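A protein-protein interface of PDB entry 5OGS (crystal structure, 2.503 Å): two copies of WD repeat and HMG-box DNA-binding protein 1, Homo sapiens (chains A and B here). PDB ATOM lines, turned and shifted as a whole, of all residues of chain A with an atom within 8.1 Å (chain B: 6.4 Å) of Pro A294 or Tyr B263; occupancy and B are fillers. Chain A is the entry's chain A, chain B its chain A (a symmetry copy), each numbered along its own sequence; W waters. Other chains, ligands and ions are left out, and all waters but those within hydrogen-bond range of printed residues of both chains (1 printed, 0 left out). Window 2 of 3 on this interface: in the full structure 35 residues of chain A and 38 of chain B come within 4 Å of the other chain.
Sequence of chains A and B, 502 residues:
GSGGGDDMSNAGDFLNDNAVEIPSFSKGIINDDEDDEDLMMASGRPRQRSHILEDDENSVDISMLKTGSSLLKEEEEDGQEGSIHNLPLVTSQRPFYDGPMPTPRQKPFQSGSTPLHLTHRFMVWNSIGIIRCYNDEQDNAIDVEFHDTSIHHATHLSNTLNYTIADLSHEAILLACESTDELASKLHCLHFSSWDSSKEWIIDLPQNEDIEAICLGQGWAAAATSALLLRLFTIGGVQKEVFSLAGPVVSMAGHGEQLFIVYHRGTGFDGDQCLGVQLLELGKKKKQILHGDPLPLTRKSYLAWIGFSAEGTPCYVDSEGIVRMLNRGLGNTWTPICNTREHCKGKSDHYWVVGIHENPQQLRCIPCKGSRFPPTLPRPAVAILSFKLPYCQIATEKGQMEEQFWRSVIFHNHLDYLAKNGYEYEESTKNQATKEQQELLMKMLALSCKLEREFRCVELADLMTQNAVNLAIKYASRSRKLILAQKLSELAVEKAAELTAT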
ATOM      1  N   TYR A 263      10.904  19.117  14.048  1.00  0.00           N
ATOM      2  CA  TYR A 263      11.635  18.824  12.826  1.00  0.00           C
ATOM      3  C   TYR A 263      11.167  19.760  11.722  1.00  0.00           C
ATOM      4  O   TYR A 263      10.190  20.499  11.874  1.00  0.00           O
ATOM      5  CB  TYR A 263      11.444  17.362  12.403  1.00  0.00           C
ATOM      6  CG  TYR A 263      10.013  17.025  12.043  1.00  0.00           C
ATOM      7  CD1 TYR A 263       9.592  17.021  10.719  1.00  0.00           C
ATOM      8  CD2 TYR A 263       9.081  16.721  13.028  1.00  0.00           C
ATOM      9  CE1 TYR A 263       8.284  16.720  10.386  1.00  0.00           C
ATOM     10  CE2 TYR A 263       7.770  16.420  12.704  1.00  0.00           C
ATOM     11  CZ  TYR A 263       7.378  16.419  11.381  1.00  0.00           C
ATOM     12  OH  TYR A 263       6.076  16.118  11.053  1.00  0.00           O
ATOM     13  N   ARG A 265       9.224  20.254   8.608  1.00  0.00           N
ATOM     14  CA  ARG A 265       8.153  19.678   7.809  1.00  0.00           C
ATOM     15  C   ARG A 265       8.096  20.256   6.400  1.00  0.00           C
ATOM     16  O   ARG A 265       7.335  19.751   5.568  1.00  0.00           O
ATOM     17  CB  ARG A 265       6.800  19.892   8.498  1.00  0.00           C
ATOM     18  CG  ARG A 265       6.401  21.351   8.633  1.00  0.00           C
ATOM     19  CD  ARG A 265       5.019  21.497   9.249  1.00  0.00           C
ATOM     20  NE  ARG A 265       4.654  22.898   9.437  1.00  0.00           N
ATOM     21  CZ  ARG A 265       3.991  23.624   8.544  1.00  0.00           C
ATOM     22  NH1 ARG A 265       3.614  23.082   7.395  1.00  0.00           N
ATOM     23  NH2 ARG A 265       3.702  24.894   8.800  1.00  0.00           N
ATOM     24  N   CYS A 274       9.725  26.359   8.682  1.00  0.00           N
ATOM     25  CA  CYS A 274       8.570  25.490   8.456  1.00  0.00           C
ATOM     26  C   CYS A 274       8.773  24.255   9.327  1.00  0.00           C
ATOM     27  O   CYS A 274       9.324  23.247   8.878  1.00  0.00           O
ATOM     28  CB  CYS A 274       8.423  25.140   6.979  1.00  0.00           C
ATOM     29  SG  CYS A 274       6.819  24.438   6.543  1.00  0.00           S
ATOM     30  N   LEU A 275       8.327  24.338  10.577  1.00  0.00           N
ATOM     31  CA  LEU A 275       8.614  23.332  11.589  1.00  0.00           C
ATOM     32  C   LEU A 275       7.359  22.543  11.941  1.00  0.00           C
ATOM     33  O   LEU A 275       6.250  23.087  11.944  1.00  0.00           O
ATOM     34  CB  LEU A 275       9.189  23.984  12.852  1.00  0.00           C
ATOM     35  CG  LEU A 275      10.711  24.100  12.981  1.00  0.00           C
ATOM     36  CD1 LEU A 275      11.382  24.405  11.649  1.00  0.00           C
ATOM     37  CD2 LEU A 275      11.081  25.142  14.025  1.00  0.00           C
ATOM     38  N   GLY A 276       7.547  21.261  12.232  1.00  0.00           N
ATOM     39  CA  GLY A 276       6.466  20.420  12.702  1.00  0.00           C
ATOM     40  C   GLY A 276       6.859  19.720  13.993  1.00  0.00           C
ATOM     41  O   GLY A 276       8.037  19.501  14.266  1.00  0.00           O
ATOM     42  N   VAL A 277       5.844  19.378  14.781  1.00  0.00           N
ATOM     43  CA  VAL A 277       6.041  18.770  16.094  1.00  0.00           C
ATOM     44  C   VAL A 277       5.423  17.380  16.095  1.00  0.00           C
ATOM     45  O   VAL A 277       4.265  17.207  15.702  1.00  0.00           O
ATOM     46  CB  VAL A 277       5.440  19.634  17.221  1.00  0.00           C
ATOM     47  CG1 VAL A 277       4.065  20.146  16.832  1.00  0.00           C
ATOM     48  CG2 VAL A 277       5.355  18.833  18.503  1.00  0.00           C
ATOM     49  N   GLN A 278       6.199  16.390  16.536  1.00  0.00           N
ATOM     50  CA  GLN A 278       5.710  15.034  16.759  1.00  0.00           C
ATOM     51  C   GLN A 278       5.832  14.735  18.248  1.00  0.00           C
ATOM     52  O   GLN A 278       6.945  14.660  18.781  1.00  0.00           O
ATOM     53  CB  GLN A 278       6.489  14.017  15.926  1.00  0.00           C
ATOM     54  CG  GLN A 278       5.866  12.631  15.922  1.00  0.00           C
ATOM     55  CD  GLN A 278       6.601  11.661  15.019  1.00  0.00           C
ATOM     56  OE1 GLN A 278       7.813  11.760  14.839  1.00  0.00           O
ATOM     57  NE2 GLN A 278       5.865  10.717  14.440  1.00  0.00           N
ATOM     58  N   LEU A 290       0.575  14.114  18.664  1.00  0.00           N
ATOM     59  CA  LEU A 290       0.608  15.081  17.573  1.00  0.00           C
ATOM     60  C   LEU A 290       1.256  14.430  16.359  1.00  0.00           C
ATOM     61  O   LEU A 290       2.434  14.060  16.405  1.00  0.00           O
ATOM     62  CB  LEU A 290       1.367  16.345  17.984  1.00  0.00           C
ATOM     63  CG  LEU A 290       0.805  17.096  19.193  1.00  0.00           C
ATOM     64  CD1 LEU A 290       1.620  18.347  19.485  1.00  0.00           C
ATOM     65  CD2 LEU A 290      -0.659  17.445  18.975  1.00  0.00           C
ATOM     66  N   HIS A 291       0.486  14.293  15.278  1.00  0.00           N
ATOM     67  CA  HIS A 291       0.966  13.658  14.050  1.00  0.00           C
ATOM     68  C   HIS A 291       1.612  14.689  13.125  1.00  0.00           C
ATOM     69  O   HIS A 291       1.178  14.928  11.999  1.00  0.00           O
ATOM     70  CB  HIS A 291      -0.179  12.933  13.348  1.00  0.00           C
ATOM     71  CG  HIS A 291      -0.716  11.765  14.112  1.00  0.00           C
ATOM     72  ND1 HIS A 291      -0.516  10.460  13.714  1.00  0.00           N
ATOM     73  CD2 HIS A 291      -1.449  11.703  15.249  1.00  0.00           C
ATOM     74  CE1 HIS A 291      -1.102   9.645  14.574  1.00  0.00           C
ATOM     75  NE2 HIS A 291      -1.674  10.374  15.515  1.00  0.00           N
ATOM     76  N   GLY A 292       2.680  15.302  13.624  1.00  0.00           N
ATOM     77  CA  GLY A 292       3.383  16.303  12.842  1.00  0.00           C
ATOM     78  C   GLY A 292       2.617  17.595  12.661  1.00  0.00           C
ATOM     79  O   GLY A 292       2.579  18.137  11.549  1.00  0.00           O
ATOM     80  N   ASP A 293       2.003  18.103  13.726  1.00  0.00           N
ATOM     81  CA  ASP A 293       1.288  19.364  13.636  1.00  0.00           C
ATOM     82  C   ASP A 293       2.264  20.500  13.340  1.00  0.00           C
ATOM     83  O   ASP A 293       3.437  20.438  13.720  1.00  0.00           O
ATOM     84  CB  ASP A 293       0.531  19.649  14.933  1.00  0.00           C
ATOM     85  CG  ASP A 293      -0.659  18.731  15.128  1.00  0.00           C
ATOM     86  OD1 ASP A 293      -0.819  17.781  14.332  1.00  0.00           O
ATOM     87  OD2 ASP A 293      -1.440  18.965  16.073  1.00  0.00           O
ATOM     88  N   PRO A 294       1.813  21.547  12.648  1.00  0.00           N
ATOM     89  CA  PRO A 294       2.689  22.701  12.407  1.00  0.00           C
ATOM     90  C   PRO A 294       3.001  23.418  13.712  1.00  0.00           C
ATOM     91  O   PRO A 294       2.110  23.667  14.528  1.00  0.00           O
ATOM     92  CB  PRO A 294       1.870  23.583  11.456  1.00  0.00           C
ATOM     93  CG  PRO A 294       0.817  22.679  10.891  1.00  0.00           C
ATOM     94  CD  PRO A 294       0.515  21.687  11.968  1.00  0.00           C
ATOM     95  N   LEU A 295       4.279  23.746  13.908  1.00  0.00           N
ATOM     96  CA  LEU A 295       4.719  24.399  15.131  1.00  0.00           C
ATOM     97  C   LEU A 295       4.603  25.911  14.959  1.00  0.00           C
ATOM     98  O   LEU A 295       5.339  26.480  14.138  1.00  0.00           O
ATOM     99  CB  LEU A 295       6.149  24.010  15.467  1.00  0.00           C
ATOM    100  CG  LEU A 295       6.609  24.413  16.867  1.00  0.00           C
ATOM    101  CD1 LEU A 295       5.850  23.617  17.917  1.00  0.00           C
ATOM    102  CD2 LEU A 295       8.107  24.227  17.020  1.00  0.00           C
ATOM    103  N   PRO A 296       3.717  26.585  15.686  1.00  0.00           N
ATOM    104  CA  PRO A 296       3.590  28.042  15.526  1.00  0.00           C
ATOM    105  C   PRO A 296       4.851  28.757  15.990  1.00  0.00           C
ATOM    106  O   PRO A 296       5.399  28.457  17.053  1.00  0.00           O
ATOM    107  CB  PRO A 296       2.386  28.395  16.409  1.00  0.00           C
ATOM    108  CG  PRO A 296       1.653  27.102  16.605  1.00  0.00           C
ATOM    109  CD  PRO A 296       2.710  26.042  16.610  1.00  0.00           C
ATOM    110  N   LEU A 297       5.307  29.709  15.179  1.00  0.00           N
ATOM    111  CA  LEU A 297       6.463  30.531  15.498  1.00  0.00           C
ATOM    112  C   LEU A 297       6.160  31.984  15.165  1.00  0.00           C
ATOM    113  O   LEU A 297       5.333  32.278  14.299  1.00  0.00           O
ATOM    114  CB  LEU A 297       7.714  30.084  14.727  1.00  0.00           C
ATOM    115  CG  LEU A 297       8.358  28.743  15.084  1.00  0.00           C
ATOM    116  CD1 LEU A 297       9.528  28.465  14.156  1.00  0.00           C
ATOM    117  CD2 LEU A 297       8.808  28.732  16.536  1.00  0.00           C
ATOM    118  N   TYR A 316       8.236  25.677  24.467  1.00  0.00           N
ATOM    119  CA  TYR A 316       9.331  26.058  23.588  1.00  0.00           C
ATOM    120  C   TYR A 316       9.393  27.573  23.471  1.00  0.00           C
ATOM    121  O   TYR A 316       8.412  28.278  23.721  1.00  0.00           O
ATOM    122  CB  TYR A 316       9.207  25.406  22.204  1.00  0.00           C
ATOM    123  CG  TYR A 316       8.018  25.843  21.380  1.00  0.00           C
ATOM    124  CD1 TYR A 316       8.150  26.810  20.391  1.00  0.00           C
ATOM    125  CD2 TYR A 316       6.767  25.271  21.572  1.00  0.00           C
ATOM    126  CE1 TYR A 316       7.068  27.205  19.627  1.00  0.00           C
ATOM    127  CE2 TYR A 316       5.680  25.659  20.813  1.00  0.00           C
ATOM    128  CZ  TYR A 316       5.835  26.626  19.842  1.00  0.00           C
ATOM    129  OH  TYR A 316       4.755  27.013  19.083  1.00  0.00           O
ATOM    130  N   ASN A 332      -5.049  20.782  22.694  1.00  0.00           N
ATOM    131  CA  ASN A 332      -3.616  20.651  22.415  1.00  0.00           C
ATOM    132  C   ASN A 332      -3.122  21.734  21.457  1.00  0.00           C
ATOM    133  O   ASN A 332      -2.302  21.481  20.571  1.00  0.00           O
ATOM    134  CB  ASN A 332      -3.273  19.258  21.879  1.00  0.00           C
ATOM    135  CG  ASN A 332      -3.315  18.196  22.955  1.00  0.00           C
ATOM    136  OD1 ASN A 332      -3.097  18.481  24.132  1.00  0.00           O
ATOM    137  ND2 ASN A 332      -3.592  16.960  22.556  1.00  0.00           N
ATOM    138  N   TRP A 334      -1.236  25.674  21.211  1.00  0.00           N
ATOM    139  CA  TRP A 334      -0.070  26.276  21.844  1.00  0.00           C
ATOM    140  C   TRP A 334      -0.405  27.704  22.251  1.00  0.00           C
ATOM    141  O   TRP A 334      -0.828  28.509  21.414  1.00  0.00           O
ATOM    142  CB  TRP A 334       1.138  26.244  20.908  1.00  0.00           C
ATOM    143  CG  TRP A 334       1.526  24.857  20.491  1.00  0.00           C
ATOM    144  CD1 TRP A 334       1.119  24.194  19.370  1.00  0.00           C
ATOM    145  CD2 TRP A 334       2.395  23.958  21.195  1.00  0.00           C
ATOM    146  NE1 TRP A 334       1.682  22.942  19.329  1.00  0.00           N
ATOM    147  CE2 TRP A 334       2.469  22.772  20.438  1.00  0.00           C
ATOM    148  CE3 TRP A 334       3.116  24.044  22.390  1.00  0.00           C
ATOM    149  CZ2 TRP A 334       3.238  21.680  20.835  1.00  0.00           C
ATOM    150  CZ3 TRP A 334       3.879  22.957  22.783  1.00  0.00           C
ATOM    151  CH2 TRP A 334       3.934  21.792  22.008  1.00  0.00           C
ATOM    152  N   LEU B 245      -1.442  30.819  16.078  1.00  0.00           N
ATOM    153  CA  LEU B 245      -1.792  30.258  14.782  1.00  0.00           C
ATOM    154  C   LEU B 245      -0.543  29.734  14.087  1.00  0.00           C
ATOM    155  O   LEU B 245       0.539  30.318  14.201  1.00  0.00           O
ATOM    156  CB  LEU B 245      -2.477  31.309  13.906  1.00  0.00           C
ATOM    157  CG  LEU B 245      -3.827  31.839  14.395  1.00  0.00           C
ATOM    158  CD1 LEU B 245      -4.233  33.077  13.611  1.00  0.00           C
ATOM    159  CD2 LEU B 245      -4.894  30.761  14.283  1.00  0.00           C
ATOM    160  N   ALA B 246      -0.699  28.624  13.364  1.00  0.00           N
ATOM    161  CA  ALA B 246       0.431  28.029  12.664  1.00  0.00           C
ATOM    162  C   ALA B 246       0.858  28.831  11.443  1.00  0.00           C
ATOM    163  O   ALA B 246       1.947  28.585  10.911  1.00  0.00           O
ATOM    164  CB  ALA B 246       0.094  26.596  12.251  1.00  0.00           C
ATOM    165  N   GLY B 247       0.039  29.775  10.991  1.00  0.00           N
ATOM    166  CA  GLY B 247       0.371  30.598   9.855  1.00  0.00           C
ATOM    167  C   GLY B 247      -0.562  31.783   9.727  1.00  0.00           C
ATOM    168  O   GLY B 247      -1.537  31.917  10.476  1.00  0.00           O
ATOM    169  N   PRO B 248      -0.276  32.673   8.780  1.00  0.00           N
ATOM    170  CA  PRO B 248      -1.146  33.840   8.574  1.00  0.00           C
ATOM    171  C   PRO B 248      -2.557  33.416   8.195  1.00  0.00           C
ATOM    172  O   PRO B 248      -2.757  32.546   7.345  1.00  0.00           O
ATOM    173  CB  PRO B 248      -0.454  34.600   7.437  1.00  0.00           C
ATOM    174  CG  PRO B 248       0.971  34.150   7.493  1.00  0.00           C
ATOM    175  CD  PRO B 248       0.917  32.713   7.918  1.00  0.00           C
ATOM    176  N   VAL B 249      -3.542  34.045   8.839  1.00  0.00           N
ATOM    177  CA  VAL B 249      -4.935  33.679   8.623  1.00  0.00           C
ATOM    178  C   VAL B 249      -5.387  34.124   7.235  1.00  0.00           C
ATOM    179  O   VAL B 249      -4.921  35.137   6.693  1.00  0.00           O
ATOM    180  CB  VAL B 249      -5.822  34.287   9.727  1.00  0.00           C
ATOM    181  CG1 VAL B 249      -5.834  35.809   9.630  1.00  0.00           C
ATOM    182  CG2 VAL B 249      -7.238  33.721   9.667  1.00  0.00           C
ATOM    183  N   VAL B 250      -6.290  33.348   6.644  1.00  0.00           N
ATOM    184  CA  VAL B 250      -6.913  33.678   5.369  1.00  0.00           C
ATOM    185  C   VAL B 250      -8.370  34.091   5.559  1.00  0.00           C
ATOM    186  O   VAL B 250      -8.805  35.121   5.044  1.00  0.00           O
ATOM    187  CB  VAL B 250      -6.795  32.502   4.375  1.00  0.00           C
ATOM    188  CG1 VAL B 250      -7.511  32.833   3.074  1.00  0.00           C
ATOM    189  CG2 VAL B 250      -5.333  32.173   4.119  1.00  0.00           C
ATOM    190  N   SER B 251      -9.138  33.294   6.295  1.00  0.00           N
ATOM    191  CA  SER B 251     -10.519  33.639   6.595  1.00  0.00           C
ATOM    192  C   SER B 251     -10.954  32.858   7.826  1.00  0.00           C
ATOM    193  O   SER B 251     -10.341  31.852   8.193  1.00  0.00           O
ATOM    194  CB  SER B 251     -11.447  33.355   5.410  1.00  0.00           C
ATOM    195  OG  SER B 251     -12.731  33.911   5.632  1.00  0.00           O
ATOM    196  N   ILE B 261     -11.140  27.933  10.904  1.00  0.00           N
ATOM    197  CA  ILE B 261      -9.993  28.771  10.572  1.00  0.00           C
ATOM    198  C   ILE B 261      -9.296  28.185   9.353  1.00  0.00           C
ATOM    199  O   ILE B 261      -8.985  26.988   9.327  1.00  0.00           O
ATOM    200  CB  ILE B 261      -9.009  28.880  11.749  1.00  0.00           C
ATOM    201  CG1 ILE B 261      -9.747  29.256  13.033  1.00  0.00           C
ATOM    202  CG2 ILE B 261      -7.916  29.895  11.437  1.00  0.00           C
ATOM    203  CD1 ILE B 261      -8.940  28.996  14.280  1.00  0.00           C
ATOM    204  N   VAL B 262      -9.044  29.026   8.355  1.00  0.00           N
ATOM    205  CA  VAL B 262      -8.235  28.670   7.198  1.00  0.00           C
ATOM    206  C   VAL B 262      -7.030  29.598   7.169  1.00  0.00           C
ATOM    207  O   VAL B 262      -7.182  30.821   7.266  1.00  0.00           O
ATOM    208  CB  VAL B 262      -9.033  28.763   5.886  1.00  0.00           C
ATOM    209  CG1 VAL B 262      -8.137  28.439   4.701  1.00  0.00           C
ATOM    210  CG2 VAL B 262     -10.228  27.825   5.932  1.00  0.00           C
ATOM    211  N   TYR B 263      -5.840  29.018   7.042  1.00  0.00           N
ATOM    212  CA  TYR B 263      -4.600  29.773   7.118  1.00  0.00           C
ATOM    213  C   TYR B 263      -3.604  29.209   6.116  1.00  0.00           C
ATOM    214  O   TYR B 263      -3.829  28.161   5.503  1.00  0.00           O
ATOM    215  CB  TYR B 263      -4.012  29.733   8.535  1.00  0.00           C
ATOM    216  CG  TYR B 263      -3.603  28.344   8.974  1.00  0.00           C
ATOM    217  CD1 TYR B 263      -2.282  27.924   8.871  1.00  0.00           C
ATOM    218  CD2 TYR B 263      -4.538  27.450   9.481  1.00  0.00           C
ATOM    219  CE1 TYR B 263      -1.904  26.653   9.266  1.00  0.00           C
ATOM    220  CE2 TYR B 263      -4.169  26.177   9.878  1.00  0.00           C
ATOM    221  CZ  TYR B 263      -2.851  25.785   9.769  1.00  0.00           C
ATOM    222  OH  TYR B 263      -2.477  24.521  10.163  1.00  0.00           O
ATOM    223  N   HIS B 264      -2.487  29.917   5.958  1.00  0.00           N
ATOM    224  CA  HIS B 264      -1.400  29.465   5.096  1.00  0.00           C
ATOM    225  C   HIS B 264      -0.526  28.490   5.875  1.00  0.00           C
ATOM    226  O   HIS B 264       0.156  28.881   6.829  1.00  0.00           O
ATOM    227  CB  HIS B 264      -0.581  30.651   4.593  1.00  0.00           C
ATOM    228  CG  HIS B 264      -1.331  31.562   3.670  1.00  0.00           C
ATOM    229  ND1 HIS B 264      -1.601  31.235   2.358  1.00  0.00           N
ATOM    230  CD2 HIS B 264      -1.859  32.793   3.866  1.00  0.00           C
ATOM    231  CE1 HIS B 264      -2.270  32.222   1.790  1.00  0.00           C
ATOM    232  NE2 HIS B 264      -2.438  33.180   2.683  1.00  0.00           N
ATOM    233  N   ARG B 265      -0.547  27.219   5.475  1.00  0.00           N
ATOM    234  CA  ARG B 265       0.324  26.212   6.064  1.00  0.00           C
ATOM    235  C   ARG B 265       1.658  26.093   5.339  1.00  0.00           C
ATOM    236  O   ARG B 265       2.550  25.387   5.822  1.00  0.00           O
ATOM    237  CB  ARG B 265      -0.372  24.846   6.070  1.00  0.00           C
ATOM    238  CG  ARG B 265      -0.667  24.298   4.685  1.00  0.00           C
ATOM    239  CD  ARG B 265      -1.282  22.909   4.752  1.00  0.00           C
ATOM    240  NE  ARG B 265      -1.623  22.402   3.427  1.00  0.00           N
ATOM    241  CZ  ARG B 265      -0.812  21.666   2.676  1.00  0.00           C
ATOM    242  NH1 ARG B 265       0.395  21.344   3.120  1.00  0.00           N
ATOM    243  NH2 ARG B 265      -1.206  21.247   1.480  1.00  0.00           N
ATOM    244  N   GLY B 266       1.810  26.756   4.204  1.00  0.00           N
ATOM    245  CA  GLY B 266       3.049  26.691   3.464  1.00  0.00           C
ATOM    246  C   GLY B 266       3.029  27.658   2.303  1.00  0.00           C
ATOM    247  O   GLY B 266       2.259  28.620   2.286  1.00  0.00           O
ATOM    248  N   CYS B 274      -1.315  27.086  -0.602  1.00  0.00           N
ATOM    249  CA  CYS B 274      -0.980  26.027   0.351  1.00  0.00           C
ATOM    250  C   CYS B 274      -1.708  26.358   1.649  1.00  0.00           C
ATOM    251  O   CYS B 274      -1.153  27.010   2.538  1.00  0.00           O
ATOM    252  CB  CYS B 274       0.528  25.914   0.545  1.00  0.00           C
ATOM    253  SG  CYS B 274       1.056  24.390   1.354  1.00  0.00           S
ATOM    254  N   LEU B 275      -2.955  25.909   1.755  1.00  0.00           N
ATOM    255  CA  LEU B 275      -3.850  26.300   2.834  1.00  0.00           C
ATOM    256  C   LEU B 275      -4.098  25.134   3.782  1.00  0.00           C
ATOM    257  O   LEU B 275      -4.151  23.974   3.360  1.00  0.00           O
ATOM    258  CB  LEU B 275      -5.183  26.806   2.274  1.00  0.00           C
ATOM    259  CG  LEU B 275      -5.340  28.309   2.017  1.00  0.00           C
ATOM    260  CD1 LEU B 275      -4.058  28.942   1.495  1.00  0.00           C
ATOM    261  CD2 LEU B 275      -6.498  28.570   1.067  1.00  0.00           C
ATOM    262  N   GLY B 276      -4.244  25.453   5.064  1.00  0.00           N
ATOM    263  CA  GLY B 276      -4.606  24.467   6.059  1.00  0.00           C
ATOM    264  C   GLY B 276      -5.813  24.932   6.857  1.00  0.00           C
ATOM    265  O   GLY B 276      -6.071  26.127   6.982  1.00  0.00           O
ATOM    266  N   VAL B 277      -6.547  23.960   7.388  1.00  0.00           N
ATOM    267  CA  VAL B 277      -7.785  24.220   8.118  1.00  0.00           C
ATOM    268  C   VAL B 277      -7.623  23.750   9.555  1.00  0.00           C
ATOM    269  O   VAL B 277      -7.201  22.615   9.800  1.00  0.00           O
ATOM    270  CB  VAL B 277      -8.996  23.536   7.453  1.00  0.00           C
ATOM    271  CG1 VAL B 277      -8.655  22.114   7.045  1.00  0.00           C
ATOM    272  CG2 VAL B 277     -10.179  23.537   8.399  1.00  0.00           C
ATOM    273  N   GLN B 278      -7.957  24.625  10.503  1.00  0.00           N
ATOM    274  CA  GLN B 278      -8.021  24.279  11.919  1.00  0.00           C
ATOM    275  C   GLN B 278      -9.467  24.434  12.370  1.00  0.00           C
ATOM    276  O   GLN B 278     -10.000  25.550  12.390  1.00  0.00           O
ATOM    277  CB  GLN B 278      -7.086  25.157  12.749  1.00  0.00           C
ATOM    278  CG  GLN B 278      -6.919  24.681  14.183  1.00  0.00           C
ATOM    279  CD  GLN B 278      -5.920  25.511  14.964  1.00  0.00           C
ATOM    280  OE1 GLN B 278      -5.765  26.706  14.721  1.00  0.00           O
ATOM    281  NE2 GLN B 278      -5.231  24.876  15.906  1.00  0.00           N
ATOM    282  N   HIS B 291      -6.414  19.157  13.021  1.00  0.00           N
ATOM    283  CA  HIS B 291      -5.127  19.697  13.461  1.00  0.00           C
ATOM    284  C   HIS B 291      -4.330  20.232  12.269  1.00  0.00           C
ATOM    285  O   HIS B 291      -3.235  19.774  11.951  1.00  0.00           O
ATOM    286  CB  HIS B 291      -4.336  18.633  14.215  1.00  0.00           C
ATOM    287  CG  HIS B 291      -4.958  18.221  15.512  1.00  0.00           C
ATOM    288  ND1 HIS B 291      -4.418  18.554  16.735  1.00  0.00           N
ATOM    289  CD2 HIS B 291      -6.074  17.500  15.777  1.00  0.00           C
ATOM    290  CE1 HIS B 291      -5.174  18.057  17.698  1.00  0.00           C
ATOM    291  NE2 HIS B 291      -6.185  17.414  17.143  1.00  0.00           N
ATOM    292  N   GLY B 292      -4.906  21.231  11.610  1.00  0.00           N
ATOM    293  CA  GLY B 292      -4.249  21.826  10.460  1.00  0.00           C
ATOM    294  C   GLY B 292      -4.208  20.931   9.242  1.00  0.00           C
ATOM    295  O   GLY B 292      -3.164  20.834   8.585  1.00  0.00           O
ATOM    296  N   ASP B 293      -5.317  20.269   8.924  1.00  0.00           N
ATOM    297  CA  ASP B 293      -5.363  19.427   7.742  1.00  0.00           C
ATOM    298  C   ASP B 293      -5.207  20.280   6.484  1.00  0.00           C
ATOM    299  O   ASP B 293      -5.589  21.454   6.468  1.00  0.00           O
ATOM    300  CB  ASP B 293      -6.677  18.648   7.685  1.00  0.00           C
ATOM    301  CG  ASP B 293      -6.754  17.559   8.737  1.00  0.00           C
ATOM    302  OD1 ASP B 293      -5.855  17.497   9.602  1.00  0.00           O
ATOM    303  OD2 ASP B 293      -7.713  16.759   8.692  1.00  0.00           O
HETATM  304  O   HOH W   1      -4.993  16.117  20.068  1.00  0.00           O
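The backbone carbonyl oxygen of Arg B265 sits at hydrogen-bond distance from the guanidinium group of Arg A265. A ring nitrogen (ND1) of His B291 lies within hydrogen-bond range of the side-chain carboxylate (OD2) of Asp A293.
NE of Arg A265 is in hydrogen-bond range of O of Leu A275 (3.0 Å). N of Val A277 lies within hydrogen-bond range of O of Asp A293 (2.8 Å). O of Pro A296 lies within hydrogen-bond range of OH of Tyr A316 (2.6 Å). N of Gly B276 sits at hydrogen-bond distance from O of Tyr B263 (2.8 Å). The backbone carbonyl oxygen (O) of Cys B274 lies within hydrogen-bond range of the backbone NH (N) of Arg B265 (3.0 Å). O of Leu B275 lies within hydrogen-bond range of NE of Arg B265 (3.0 Å).
Among the printed residues, pairs that only touch across the chains: Pro A294 with Ala B246, Pro A294 with Tyr B263 and Pro A296 with Leu B245.
Pro A294 touches two residues of chain B. Tyr B263 touches just one residue of chain A: Pro A294 (3.8 Å). No residue of chain A comes within 4 Å of Gly B276. Printed residues of chain B within 4 Å of Pro A296: Leu B245. Printed residues of chain A within 4 Å of His B291: Asp A293. Of the printed residues of chain B, Asp A293 touches His B291. Of the printed residues of chain A, Leu B245 touches Pro A296. Of the printed residues of chain B, Arg A265 touches Arg B265 (3.0 Å). Leu A297 touches none of the printed residues of chain B. Val B249 touches none of the printed residues of chain A. The nearest residue of chain B that does not touch Pro A294 is His B291 (4.2 Å). The nearest residue of chain A that does not touch Tyr B263 is Arg A265 (5.9 Å).
Hydrophobic or aromatic side chains of chain A that line the printed part of chain B: Pro A294 and Pro A296. Among the printed residues, 5 pairs touch across the chains. Among the printed residues, no Asp or Glu carboxylate lies within 4 Å of a Lys or Arg side-chain nitrogen of the other chain.
Arg A265 touches its own counterpart, Arg B265. Asp A293 touches His B291, but with the chains exchanged His A291 does not touch Asp B293 (7.9 Å). 10 positions are printed for both chains. Of the 5 pairs that touch across the chains among the printed residues, 1 has its exchanged pair printed and touching as well.
Water W1 bridges ND2 of Asn A332 and NE2 of His B291.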
